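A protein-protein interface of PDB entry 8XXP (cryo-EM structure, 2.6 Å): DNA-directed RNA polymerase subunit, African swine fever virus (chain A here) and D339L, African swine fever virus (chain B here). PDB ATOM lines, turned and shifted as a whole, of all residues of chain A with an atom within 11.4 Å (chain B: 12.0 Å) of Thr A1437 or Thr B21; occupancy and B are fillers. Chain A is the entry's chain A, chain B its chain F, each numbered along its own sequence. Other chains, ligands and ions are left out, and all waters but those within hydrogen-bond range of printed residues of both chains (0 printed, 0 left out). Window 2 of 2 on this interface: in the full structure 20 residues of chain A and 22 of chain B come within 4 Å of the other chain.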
ATOM      1  N   MET A1431       2.314  14.513  15.673  1.00  0.00           N
ATOM      2  CA  MET A1431       2.914  14.923  14.417  1.00  0.00           C
ATOM      3  C   MET A1431       4.428  14.986  14.566  1.00  0.00           C
ATOM      4  O   MET A1431       4.949  15.491  15.562  1.00  0.00           O
ATOM      5  CB  MET A1431       2.364  16.283  13.996  1.00  0.00           C
ATOM      6  CG  MET A1431       0.871  16.287  13.721  1.00  0.00           C
ATOM      7  SD  MET A1431       0.318  15.528  12.190  1.00  0.00           S
ATOM      8  CE  MET A1431       1.582  16.055  11.058  1.00  0.00           C
ATOM      9  N   ASP A1432       5.139  14.464  13.570  1.00  0.00           N
ATOM     10  CA  ASP A1432       6.601  14.488  13.569  1.00  0.00           C
ATOM     11  C   ASP A1432       7.060  15.865  13.112  1.00  0.00           C
ATOM     12  O   ASP A1432       7.240  16.123  11.923  1.00  0.00           O
ATOM     13  CB  ASP A1432       7.161  13.394  12.673  1.00  0.00           C
ATOM     14  CG  ASP A1432       8.549  12.964  13.082  1.00  0.00           C
ATOM     15  OD1 ASP A1432       9.180  13.668  13.894  1.00  0.00           O
ATOM     16  OD2 ASP A1432       9.019  11.923  12.587  1.00  0.00           O
ATOM     17  N   GLU A1433       7.249  16.766  14.074  1.00  0.00           N
ATOM     18  CA  GLU A1433       7.678  18.119  13.742  1.00  0.00           C
ATOM     19  C   GLU A1433       9.074  18.126  13.134  1.00  0.00           C
ATOM     20  O   GLU A1433       9.330  18.852  12.168  1.00  0.00           O
ATOM     21  CB  GLU A1433       7.637  19.000  14.987  1.00  0.00           C
ATOM     22  CG  GLU A1433       6.270  19.117  15.615  1.00  0.00           C
ATOM     23  CD  GLU A1433       6.337  19.207  17.120  1.00  0.00           C
ATOM     24  OE1 GLU A1433       7.349  19.721  17.638  1.00  0.00           O
ATOM     25  OE2 GLU A1433       5.381  18.765  17.789  1.00  0.00           O
ATOM     26  N   LYS A1434       9.987  17.327  13.687  1.00  0.00           N
ATOM     27  CA  LYS A1434      11.348  17.281  13.165  1.00  0.00           C
ATOM     28  C   LYS A1434      11.369  16.807  11.720  1.00  0.00           C
ATOM     29  O   LYS A1434      12.086  17.367  10.884  1.00  0.00           O
ATOM     30  CB  LYS A1434      12.205  16.373  14.041  1.00  0.00           C
ATOM     31  CG  LYS A1434      13.470  15.867  13.377  1.00  0.00           C
ATOM     32  CD  LYS A1434      14.273  14.997  14.329  1.00  0.00           C
ATOM     33  CE  LYS A1434      14.717  15.780  15.557  1.00  0.00           C
ATOM     34  NZ  LYS A1434      15.120  17.176  15.227  1.00  0.00           N
ATOM     35  N   TYR A1435      10.587  15.778  11.406  1.00  0.00           N
ATOM     36  CA  TYR A1435      10.533  15.275  10.039  1.00  0.00           C
ATOM     37  C   TYR A1435       9.883  16.279   9.100  1.00  0.00           C
ATOM     38  O   TYR A1435      10.286  16.403   7.939  1.00  0.00           O
ATOM     39  CB  TYR A1435       9.777  13.953  10.008  1.00  0.00           C
ATOM     40  CG  TYR A1435       9.872  13.231   8.697  1.00  0.00           C
ATOM     41  CD1 TYR A1435      11.028  12.562   8.345  1.00  0.00           C
ATOM     42  CD2 TYR A1435       8.806  13.212   7.814  1.00  0.00           C
ATOM     43  CE1 TYR A1435      11.123  11.898   7.154  1.00  0.00           C
ATOM     44  CE2 TYR A1435       8.893  12.551   6.618  1.00  0.00           C
ATOM     45  CZ  TYR A1435      10.054  11.896   6.294  1.00  0.00           C
ATOM     46  OH  TYR A1435      10.162  11.232   5.102  1.00  0.00           O
ATOM     47  N   ILE A1436       8.864  16.992   9.578  1.00  0.00           N
ATOM     48  CA  ILE A1436       8.125  17.911   8.721  1.00  0.00           C
ATOM     49  C   ILE A1436       8.967  19.132   8.376  1.00  0.00           C
ATOM     50  O   ILE A1436       9.009  19.565   7.219  1.00  0.00           O
ATOM     51  CB  ILE A1436       6.802  18.303   9.398  1.00  0.00           C
ATOM     52  CG1 ILE A1436       5.774  17.193   9.215  1.00  0.00           C
ATOM     53  CG2 ILE A1436       6.277  19.602   8.840  1.00  0.00           C
ATOM     54  CD1 ILE A1436       4.704  17.220  10.243  1.00  0.00           C
ATOM     55  N   THR A1437       9.647  19.710   9.368  1.00  0.00           N
ATOM     56  CA  THR A1437      10.467  20.888   9.107  1.00  0.00           C
ATOM     57  C   THR A1437      11.612  20.572   8.155  1.00  0.00           C
ATOM     58  O   THR A1437      12.099  21.461   7.450  1.00  0.00           O
ATOM     59  CB  THR A1437      11.013  21.453  10.418  1.00  0.00           C
ATOM     60  OG1 THR A1437      11.780  20.450  11.090  1.00  0.00           O
ATOM     61  CG2 THR A1437       9.881  21.877  11.318  1.00  0.00           C
ATOM     62  N   GLU A1438      12.056  19.317   8.124  1.00  0.00           N
ATOM     63  CA  GLU A1438      13.142  18.900   7.251  1.00  0.00           C
ATOM     64  C   GLU A1438      12.670  18.428   5.887  1.00  0.00           C
ATOM     65  O   GLU A1438      13.508  18.190   5.012  1.00  0.00           O
ATOM     66  CB  GLU A1438      13.937  17.775   7.912  1.00  0.00           C
ATOM     67  CG  GLU A1438      14.682  18.187   9.161  1.00  0.00           C
ATOM     68  CD  GLU A1438      15.170  16.993   9.951  1.00  0.00           C
ATOM     69  OE1 GLU A1438      14.923  15.854   9.510  1.00  0.00           O
ATOM     70  OE2 GLU A1438      15.801  17.191  11.010  1.00  0.00           O
ATOM     71  N   ASN A1439      11.363  18.263   5.683  1.00  0.00           N
ATOM     72  CA  ASN A1439      10.877  17.707   4.427  1.00  0.00           C
ATOM     73  C   ASN A1439       9.732  18.514   3.827  1.00  0.00           C
ATOM     74  O   ASN A1439       9.586  18.570   2.603  1.00  0.00           O
ATOM     75  CB  ASN A1439      10.441  16.257   4.635  1.00  0.00           C
ATOM     76  CG  ASN A1439      11.562  15.380   5.151  1.00  0.00           C
ATOM     77  OD1 ASN A1439      12.262  14.730   4.380  1.00  0.00           O
ATOM     78  ND2 ASN A1439      11.748  15.370   6.461  1.00  0.00           N
ATOM     79  N   TYR A1440       8.921  19.147   4.673  1.00  0.00           N
ATOM     80  CA  TYR A1440       7.686  19.782   4.229  1.00  0.00           C
ATOM     81  C   TYR A1440       7.754  21.303   4.211  1.00  0.00           C
ATOM     82  O   TYR A1440       6.856  21.937   3.648  1.00  0.00           O
ATOM     83  CB  TYR A1440       6.514  19.335   5.114  1.00  0.00           C
ATOM     84  CG  TYR A1440       6.092  17.901   4.892  1.00  0.00           C
ATOM     85  CD1 TYR A1440       6.858  16.849   5.372  1.00  0.00           C
ATOM     86  CD2 TYR A1440       4.931  17.599   4.198  1.00  0.00           C
ATOM     87  CE1 TYR A1440       6.483  15.541   5.166  1.00  0.00           C
ATOM     88  CE2 TYR A1440       4.546  16.292   3.987  1.00  0.00           C
ATOM     89  CZ  TYR A1440       5.327  15.267   4.473  1.00  0.00           C
ATOM     90  OH  TYR A1440       4.950  13.961   4.266  1.00  0.00           O
ATOM     91  N   LYS A1441       8.780  21.902   4.804  1.00  0.00           N
ATOM     92  CA  LYS A1441       8.882  23.358   4.882  1.00  0.00           C
ATOM     93  C   LYS A1441       8.934  23.995   3.497  1.00  0.00           C
ATOM     94  O   LYS A1441       7.961  24.598   3.044  1.00  0.00           O
ATOM     95  CB  LYS A1441      10.116  23.765   5.688  1.00  0.00           C
ATOM     96  CG  LYS A1441      10.225  25.258   5.947  1.00  0.00           C
ATOM     97  CD  LYS A1441      11.528  25.601   6.653  1.00  0.00           C
ATOM     98  CE  LYS A1441      11.654  27.092   6.908  1.00  0.00           C
ATOM     99  NZ  LYS A1441      10.698  27.554   7.952  1.00  0.00           N
ATOM    100  N   ILE B  13      -5.623  22.679  16.022  1.00  0.00           N
ATOM    101  CA  ILE B  13      -4.770  22.777  14.851  1.00  0.00           C
ATOM    102  C   ILE B  13      -5.503  22.111  13.695  1.00  0.00           C
ATOM    103  O   ILE B  13      -5.528  20.884  13.580  1.00  0.00           O
ATOM    104  CB  ILE B  13      -3.401  22.147  15.106  1.00  0.00           C
ATOM    105  CG1 ILE B  13      -2.769  22.809  16.328  1.00  0.00           C
ATOM    106  CG2 ILE B  13      -2.525  22.314  13.908  1.00  0.00           C
ATOM    107  CD1 ILE B  13      -1.676  22.023  16.946  1.00  0.00           C
ATOM    108  N   ASP B  14      -6.101  22.933  12.833  1.00  0.00           N
ATOM    109  CA  ASP B  14      -6.877  22.448  11.701  1.00  0.00           C
ATOM    110  C   ASP B  14      -6.013  21.944  10.556  1.00  0.00           C
ATOM    111  O   ASP B  14      -6.475  21.112   9.771  1.00  0.00           O
ATOM    112  CB  ASP B  14      -7.796  23.556  11.199  1.00  0.00           C
ATOM    113  CG  ASP B  14      -8.315  24.425  12.323  1.00  0.00           C
ATOM    114  OD1 ASP B  14      -9.116  23.926  13.141  1.00  0.00           O
ATOM    115  OD2 ASP B  14      -7.911  25.603  12.397  1.00  0.00           O
ATOM    116  N   ASP B  15      -4.778  22.425  10.441  1.00  0.00           N
ATOM    117  CA  ASP B  15      -3.826  21.959   9.434  1.00  0.00           C
ATOM    118  C   ASP B  15      -2.561  21.544  10.167  1.00  0.00           C
ATOM    119  O   ASP B  15      -1.582  22.298  10.218  1.00  0.00           O
ATOM    120  CB  ASP B  15      -3.546  23.037   8.387  1.00  0.00           C
ATOM    121  CG  ASP B  15      -2.944  22.474   7.114  1.00  0.00           C
ATOM    122  OD1 ASP B  15      -2.216  21.465   7.188  1.00  0.00           O
ATOM    123  OD2 ASP B  15      -3.203  23.040   6.034  1.00  0.00           O
ATOM    124  N   PRO B  16      -2.558  20.354  10.773  1.00  0.00           N
ATOM    125  CA  PRO B  16      -1.387  19.930  11.559  1.00  0.00           C
ATOM    126  C   PRO B  16      -0.133  19.713  10.737  1.00  0.00           C
ATOM    127  O   PRO B  16       0.969  19.778  11.294  1.00  0.00           O
ATOM    128  CB  PRO B  16      -1.863  18.632  12.220  1.00  0.00           C
ATOM    129  CG  PRO B  16      -2.985  18.169  11.388  1.00  0.00           C
ATOM    130  CD  PRO B  16      -3.648  19.371  10.831  1.00  0.00           C
ATOM    131  N   THR B  17      -0.252  19.452   9.436  1.00  0.00           N
ATOM    132  CA  THR B  17       0.939  19.316   8.606  1.00  0.00           C
ATOM    133  C   THR B  17       1.595  20.668   8.371  1.00  0.00           C
ATOM    134  O   THR B  17       2.819  20.803   8.470  1.00  0.00           O
ATOM    135  CB  THR B  17       0.582  18.658   7.276  1.00  0.00           C
ATOM    136  OG1 THR B  17      -0.404  17.641   7.494  1.00  0.00           O
ATOM    137  CG2 THR B  17       1.818  18.038   6.645  1.00  0.00           C
ATOM    138  N   ASN B  18       0.791  21.684   8.057  1.00  0.00           N
ATOM    139  CA  ASN B  18       1.332  23.018   7.824  1.00  0.00           C
ATOM    140  C   ASN B  18       1.786  23.667   9.124  1.00  0.00           C
ATOM    141  O   ASN B  18       2.780  24.398   9.144  1.00  0.00           O
ATOM    142  CB  ASN B  18       0.285  23.876   7.110  1.00  0.00           C
ATOM    143  CG  ASN B  18       0.615  25.355   7.130  1.00  0.00           C
ATOM    144  OD1 ASN B  18       0.496  26.023   8.156  1.00  0.00           O
ATOM    145  ND2 ASN B  18       1.032  25.874   5.985  1.00  0.00           N
ATOM    146  N   PHE B  19       1.068  23.415  10.219  1.00  0.00           N
ATOM    147  CA  PHE B  19       1.413  24.023  11.499  1.00  0.00           C
ATOM    148  C   PHE B  19       2.786  23.578  11.971  1.00  0.00           C
ATOM    149  O   PHE B  19       3.564  24.384  12.491  1.00  0.00           O
ATOM    150  CB  PHE B  19       0.351  23.671  12.538  1.00  0.00           C
ATOM    151  CG  PHE B  19       0.559  24.311  13.881  1.00  0.00           C
ATOM    152  CD1 PHE B  19       1.310  23.681  14.855  1.00  0.00           C
ATOM    153  CD2 PHE B  19      -0.026  25.524  14.180  1.00  0.00           C
ATOM    154  CE1 PHE B  19       1.495  24.259  16.089  1.00  0.00           C
ATOM    155  CE2 PHE B  19       0.155  26.104  15.416  1.00  0.00           C
ATOM    156  CZ  PHE B  19       0.918  25.469  16.371  1.00  0.00           C
ATOM    157  N   CYS B  20       3.103  22.300  11.803  1.00  0.00           N
ATOM    158  CA  CYS B  20       4.356  21.756  12.306  1.00  0.00           C
ATOM    159  C   CYS B  20       5.561  22.157  11.469  1.00  0.00           C
ATOM    160  O   CYS B  20       6.693  21.915  11.896  1.00  0.00           O
ATOM    161  CB  CYS B  20       4.260  20.234  12.392  1.00  0.00           C
ATOM    162  SG  CYS B  20       3.154  19.674  13.699  1.00  0.00           S
ATOM    163  N   THR B  21       5.347  22.760  10.298  1.00  0.00           N
ATOM    164  CA  THR B  21       6.463  23.274   9.514  1.00  0.00           C
ATOM    165  C   THR B  21       7.230  24.345  10.276  1.00  0.00           C
ATOM    166  O   THR B  21       8.449  24.467  10.122  1.00  0.00           O
ATOM    167  CB  THR B  21       5.956  23.830   8.186  1.00  0.00           C
ATOM    168  OG1 THR B  21       4.925  24.788   8.438  1.00  0.00           O
ATOM    169  CG2 THR B  21       5.403  22.723   7.320  1.00  0.00           C
ATOM    170  N   ASN B  22       6.534  25.137  11.086  1.00  0.00           N
ATOM    171  CA  ASN B  22       7.174  26.101  11.981  1.00  0.00           C
ATOM    172  C   ASN B  22       6.260  26.221  13.201  1.00  0.00           C
ATOM    173  O   ASN B  22       5.299  26.992  13.200  1.00  0.00           O
ATOM    174  CB  ASN B  22       7.397  27.439  11.295  1.00  0.00           C
ATOM    175  CG  ASN B  22       8.305  28.356  12.084  1.00  0.00           C
ATOM    176  OD1 ASN B  22       8.820  27.987  13.139  1.00  0.00           O
ATOM    177  ND2 ASN B  22       8.527  29.554  11.562  1.00  0.00           N
ATOM    178  N   VAL B  23       6.566  25.434  14.232  1.00  0.00           N
ATOM    179  CA  VAL B  23       5.655  25.316  15.364  1.00  0.00           C
ATOM    180  C   VAL B  23       5.634  26.600  16.181  1.00  0.00           C
ATOM    181  O   VAL B  23       4.570  27.060  16.597  1.00  0.00           O
ATOM    182  CB  VAL B  23       6.027  24.095  16.225  1.00  0.00           C
ATOM    183  CG1 VAL B  23       5.617  24.308  17.673  1.00  0.00           C
ATOM    184  CG2 VAL B  23       5.370  22.848  15.672  1.00  0.00           C
ATOM    185  N   GLU B  24       6.799  27.199  16.425  1.00  0.00           N
ATOM    186  CA  GLU B  24       6.848  28.359  17.311  1.00  0.00           C
ATOM    187  C   GLU B  24       6.183  29.580  16.687  1.00  0.00           C
ATOM    188  O   GLU B  24       5.414  30.282  17.355  1.00  0.00           O
ATOM    189  CB  GLU B  24       8.295  28.666  17.690  1.00  0.00           C
ATOM    190  CG  GLU B  24       8.869  27.715  18.727  1.00  0.00           C
ATOM    191  CD  GLU B  24       7.940  27.499  19.912  1.00  0.00           C
ATOM    192  OE1 GLU B  24       7.368  28.489  20.415  1.00  0.00           O
ATOM    193  OE2 GLU B  24       7.783  26.339  20.343  1.00  0.00           O
ATOM    194  N   ALA B  25       6.460  29.852  15.411  1.00  0.00           N
ATOM    195  CA  ALA B  25       5.874  31.022  14.767  1.00  0.00           C
ATOM    196  C   ALA B  25       4.361  30.891  14.656  1.00  0.00           C
ATOM    197  O   ALA B  25       3.620  31.820  14.997  1.00  0.00           O
ATOM    198  CB  ALA B  25       6.496  31.232  13.389  1.00  0.00           C
ATOM    199  N   HIS B  26       3.887  29.737  14.185  1.00  0.00           N
ATOM    200  CA  HIS B  26       2.449  29.511  14.082  1.00  0.00           C
ATOM    201  C   HIS B  26       1.791  29.510  15.452  1.00  0.00           C
ATOM    202  O   HIS B  26       0.658  29.979  15.601  1.00  0.00           O
ATOM    203  CB  HIS B  26       2.182  28.193  13.366  1.00  0.00           C
ATOM    204  CG  HIS B  26       2.709  28.148  11.969  1.00  0.00           C
ATOM    205  ND1 HIS B  26       3.506  27.122  11.510  1.00  0.00           N
ATOM    206  CD2 HIS B  26       2.547  28.994  10.926  1.00  0.00           C
ATOM    207  CE1 HIS B  26       3.814  27.340  10.244  1.00  0.00           C
ATOM    208  NE2 HIS B  26       3.244  28.470   9.865  1.00  0.00           N
ATOM    209  N   LEU B  27       2.491  28.995  16.459  1.00  0.00           N
ATOM    210  CA  LEU B  27       1.955  28.944  17.810  1.00  0.00           C
ATOM    211  C   LEU B  27       1.772  30.344  18.376  1.00  0.00           C
ATOM    212  O   LEU B  27       0.726  30.661  18.953  1.00  0.00           O
ATOM    213  CB  LEU B  27       2.892  28.120  18.690  1.00  0.00           C
ATOM    214  CG  LEU B  27       2.415  27.828  20.101  1.00  0.00           C
ATOM    215  CD1 LEU B  27       1.235  26.917  19.974  1.00  0.00           C
ATOM    216  CD2 LEU B  27       3.509  27.176  20.906  1.00  0.00           C
ATOM    217  N   LEU B  28       2.786  31.196  18.223  1.00  0.00           N
ATOM    218  CA  LEU B  28       2.658  32.578  18.663  1.00  0.00           C
ATOM    219  C   LEU B  28       1.578  33.302  17.875  1.00  0.00           C
ATOM    220  O   LEU B  28       0.833  34.113  18.433  1.00  0.00           O
ATOM    221  CB  LEU B  28       3.993  33.305  18.529  1.00  0.00           C
ATOM    222  CG  LEU B  28       4.731  33.563  19.839  1.00  0.00           C
ATOM    223  CD1 LEU B  28       3.930  34.495  20.728  1.00  0.00           C
ATOM    224  CD2 LEU B  28       5.007  32.258  20.543  1.00  0.00           C
ATOM    225  N   LYS B  29       1.478  33.020  16.574  1.00  0.00           N
ATOM    226  CA  LYS B  29       0.433  33.627  15.762  1.00  0.00           C
ATOM    227  C   LYS B  29      -0.950  33.275  16.296  1.00  0.00           C
ATOM    228  O   LYS B  29      -1.811  34.146  16.446  1.00  0.00           O
ATOM    229  CB  LYS B  29       0.585  33.177  14.311  1.00  0.00           C
ATOM    230  CG  LYS B  29      -0.289  33.928  13.325  1.00  0.00           C
ATOM    231  CD  LYS B  29      -0.313  33.303  11.922  1.00  0.00           C
ATOM    232  CE  LYS B  29       0.930  32.487  11.540  1.00  0.00           C
ATOM    233  NZ  LYS B  29       2.252  33.133  11.816  1.00  0.00           N
ATOM    234  N   GLU B  30      -1.170  31.998  16.609  1.00  0.00           N
ATOM    235  CA  GLU B  30      -2.479  31.573  17.095  1.00  0.00           C
ATOM    236  C   GLU B  30      -2.768  32.117  18.489  1.00  0.00           C
ATOM    237  O   GLU B  30      -3.896  32.533  18.775  1.00  0.00           O
ATOM    238  CB  GLU B  30      -2.573  30.048  17.076  1.00  0.00           C
ATOM    239  CG  GLU B  30      -2.944  29.446  15.721  1.00  0.00           C
ATOM    240  CD  GLU B  30      -4.023  30.218  14.966  1.00  0.00           C
ATOM    241  OE1 GLU B  30      -4.015  30.172  13.719  1.00  0.00           O
ATOM    242  OE2 GLU B  30      -4.916  30.813  15.603  1.00  0.00           O
ATOM    243  N   ARG B  54       5.039  23.636  25.940  1.00  0.00           N
ATOM    244  CA  ARG B  54       4.105  23.251  24.903  1.00  0.00           C
ATOM    245  C   ARG B  54       4.142  21.738  24.802  1.00  0.00           C
ATOM    246  O   ARG B  54       5.070  21.088  25.283  1.00  0.00           O
ATOM    247  CB  ARG B  54       4.450  23.968  23.593  1.00  0.00           C
ATOM    248  CG  ARG B  54       5.713  23.469  22.904  1.00  0.00           C
ATOM    249  CD  ARG B  54       5.671  23.646  21.404  1.00  0.00           C
ATOM    250  NE  ARG B  54       4.966  22.582  20.707  1.00  0.00           N
ATOM    251  CZ  ARG B  54       5.570  21.597  20.057  1.00  0.00           C
ATOM    252  NH1 ARG B  54       6.887  21.515  19.999  1.00  0.00           N
ATOM    253  NH2 ARG B  54       4.833  20.682  19.436  1.00  0.00           N
ATOM    254  N   SER B  55       3.118  21.177  24.197  1.00  0.00           N
ATOM    255  CA  SER B  55       2.988  19.744  24.045  1.00  0.00           C
ATOM    256  C   SER B  55       3.283  19.358  22.614  1.00  0.00           C
ATOM    257  O   SER B  55       3.325  20.210  21.723  1.00  0.00           O
ATOM    258  CB  SER B  55       1.576  19.297  24.422  1.00  0.00           C
ATOM    259  OG  SER B  55       0.672  19.559  23.368  1.00  0.00           O
ATOM    260  N   PRO B  56       3.506  18.076  22.347  1.00  0.00           N
ATOM    261  CA  PRO B  56       3.494  17.621  20.958  1.00  0.00           C
ATOM    262  C   PRO B  56       2.134  17.881  20.329  1.00  0.00           C
ATOM    263  O   PRO B  56       1.112  17.991  21.007  1.00  0.00           O
ATOM    264  CB  PRO B  56       3.780  16.121  21.072  1.00  0.00           C
ATOM    265  CG  PRO B  56       4.474  15.971  22.354  1.00  0.00           C
ATOM    266  CD  PRO B  56       3.916  17.004  23.269  1.00  0.00           C
ATOM    267  N   CYS B  57       2.131  18.000  19.004  1.00  0.00           N
ATOM    268  CA  CYS B  57       0.889  18.164  18.258  1.00  0.00           C
ATOM    269  C   CYS B  57       0.159  16.826  18.252  1.00  0.00           C
ATOM    270  O   CYS B  57       0.234  16.037  17.310  1.00  0.00           O
ATOM    271  CB  CYS B  57       1.159  18.653  16.843  1.00  0.00           C
ATOM    272  SG  CYS B  57      -0.333  18.966  15.882  1.00  0.00           S
ATOM    273  N   ILE B  59      -2.811  14.319  17.774  1.00  0.00           N
ATOM    274  CA  ILE B  59      -3.918  14.235  16.831  1.00  0.00           C
ATOM    275  C   ILE B  59      -5.184  13.948  17.618  1.00  0.00           C
ATOM    276  O   ILE B  59      -5.178  13.108  18.523  1.00  0.00           O
ATOM    277  CB  ILE B  59      -3.660  13.150  15.772  1.00  0.00           C
ATOM    278  CG1 ILE B  59      -2.425  13.501  14.946  1.00  0.00           C
ATOM    279  CG2 ILE B  59      -4.863  12.986  14.865  1.00  0.00           C
ATOM    280  CD1 ILE B  59      -2.440  14.895  14.416  1.00  0.00           C
ATOM    281  N   MET B  70      -2.512  20.311  20.658  1.00  0.00           N
ATOM    282  CA  MET B  70      -1.399  20.967  21.353  1.00  0.00           C
ATOM    283  C   MET B  70      -1.840  21.748  22.588  1.00  0.00           C
ATOM    284  O   MET B  70      -2.751  22.572  22.519  1.00  0.00           O
ATOM    285  CB  MET B  70      -0.625  21.926  20.437  1.00  0.00           C
ATOM    286  CG  MET B  70       0.702  22.379  21.019  1.00  0.00           C
ATOM    287  SD  MET B  70       1.935  22.881  19.819  1.00  0.00           S
ATOM    288  CE  MET B  70       1.671  21.679  18.537  1.00  0.00           C
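The backbone NH (N) of Met A1431 lies within hydrogen-bond range of the backbone carbonyl oxygen (O) of Cys B57.
The side-chain carboxylate (OE2) of Glu A1433 lies within salt-bridge range of the guanidinium group (NH2) of Arg B54 (2.6 Å).
The side-chain hydroxyl of Thr A1437 lies within hydrogen-bond range of the backbone carbonyl oxygen of Glu A1433 (3.1 Å).
The side-chain hydroxyl of Thr A1437 lies within hydrogen-bond range of the backbone carbonyl oxygen of Lys A1434, 3.1 Å away.
The backbone carbonyl oxygen (O) of Ile A1436 sits at hydrogen-bond distance from the backbone NH (N) of Lys A1441 (3.4 Å).
O of Pro B16 is in hydrogen-bond range of SG of Cys B20.
NE of Arg B54 sits at hydrogen-bond distance from SD of Met B70.
CE of Met A1431 touches O of Pro B16, 3.8 Å away.
Met A1431 touches Cys B20.
SD of Met A1431 touches CD1 of Ile B59, 3.6 Å away.
Cys B20 touches Glu A1433.
Glu A1433 touches Pro B56 (OE2 to CA, 3.9 Å).
Glu A1433 touches Cys B57.
Ile A1436 touches Thr B17.
CB of Cys B20 touches CD1 of Ile A1436 (3.7 Å).
Ile A1436 touches Thr B21.
CD2 of Tyr A1440 touches CG2 of Thr B17, 3.98 Å away.
Thr A1437 touches just these residues of chain B: Cys B20 (3.2 Å) and Thr B21 (3.2 Å).
Of chain A, only Ile A1436 (3.6 Å) and Thr A1437 (3.2 Å) come within 4 Å of Thr B21.
No residue of chain B comes within 4 Å of Lys A1434.
Ile A1436 touches three residues of chain B.
Glu A1438 touches none of the printed residues of chain B.
No residue of chain B comes within 4 Å of Asn A1439.
No residue of chain A comes within 4 Å of Asn B18.
Of chain A, only Met A1431, Glu A1433, Ile A1436 and Thr A1437 come within 4 Å of Cys B20.
No residue of chain A comes within 4 Å of Asn B22.
Of the printed residues of chain B, Met A1431 touches Pro B16 (3.8 Å), Cys B20 (3.5 Å), Cys B57 (3.1 Å) and Ile B59 (3.6 Å).
Printed residues of chain B within 4 Å of Glu A1433: Cys B20, Val B23, Arg B54, Pro B56 and Cys B57.
Of the printed residues of chain A, Arg B54 touches Glu A1433 (2.6 Å).
Of the printed residues of chain A, Thr B17 touches Ile A1436 (3.7 Å) and Tyr A1440 (3.98 Å).
Printed residues of chain A within 4 Å of Val B23: Glu A1433 (3.8 Å).
Lys B29 touches none of the printed residues of chain A.
Glu B24 touches none of the printed residues of chain A.
Printed residues of chain B that touch a printed residue of chain A: Pro B16, Thr B17, Cys B20, Thr B21, Val B23, Arg B54, Pro B56, Cys B57 and Ile B59.
Among the printed residues, 15 pairs touch across the chains.
Among the printed residues, Asp or Glu carboxylates within 4 Å of a Lys or Arg side-chain nitrogen of the other chain: Glu A1433 with Arg B54 (2.6 Å).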
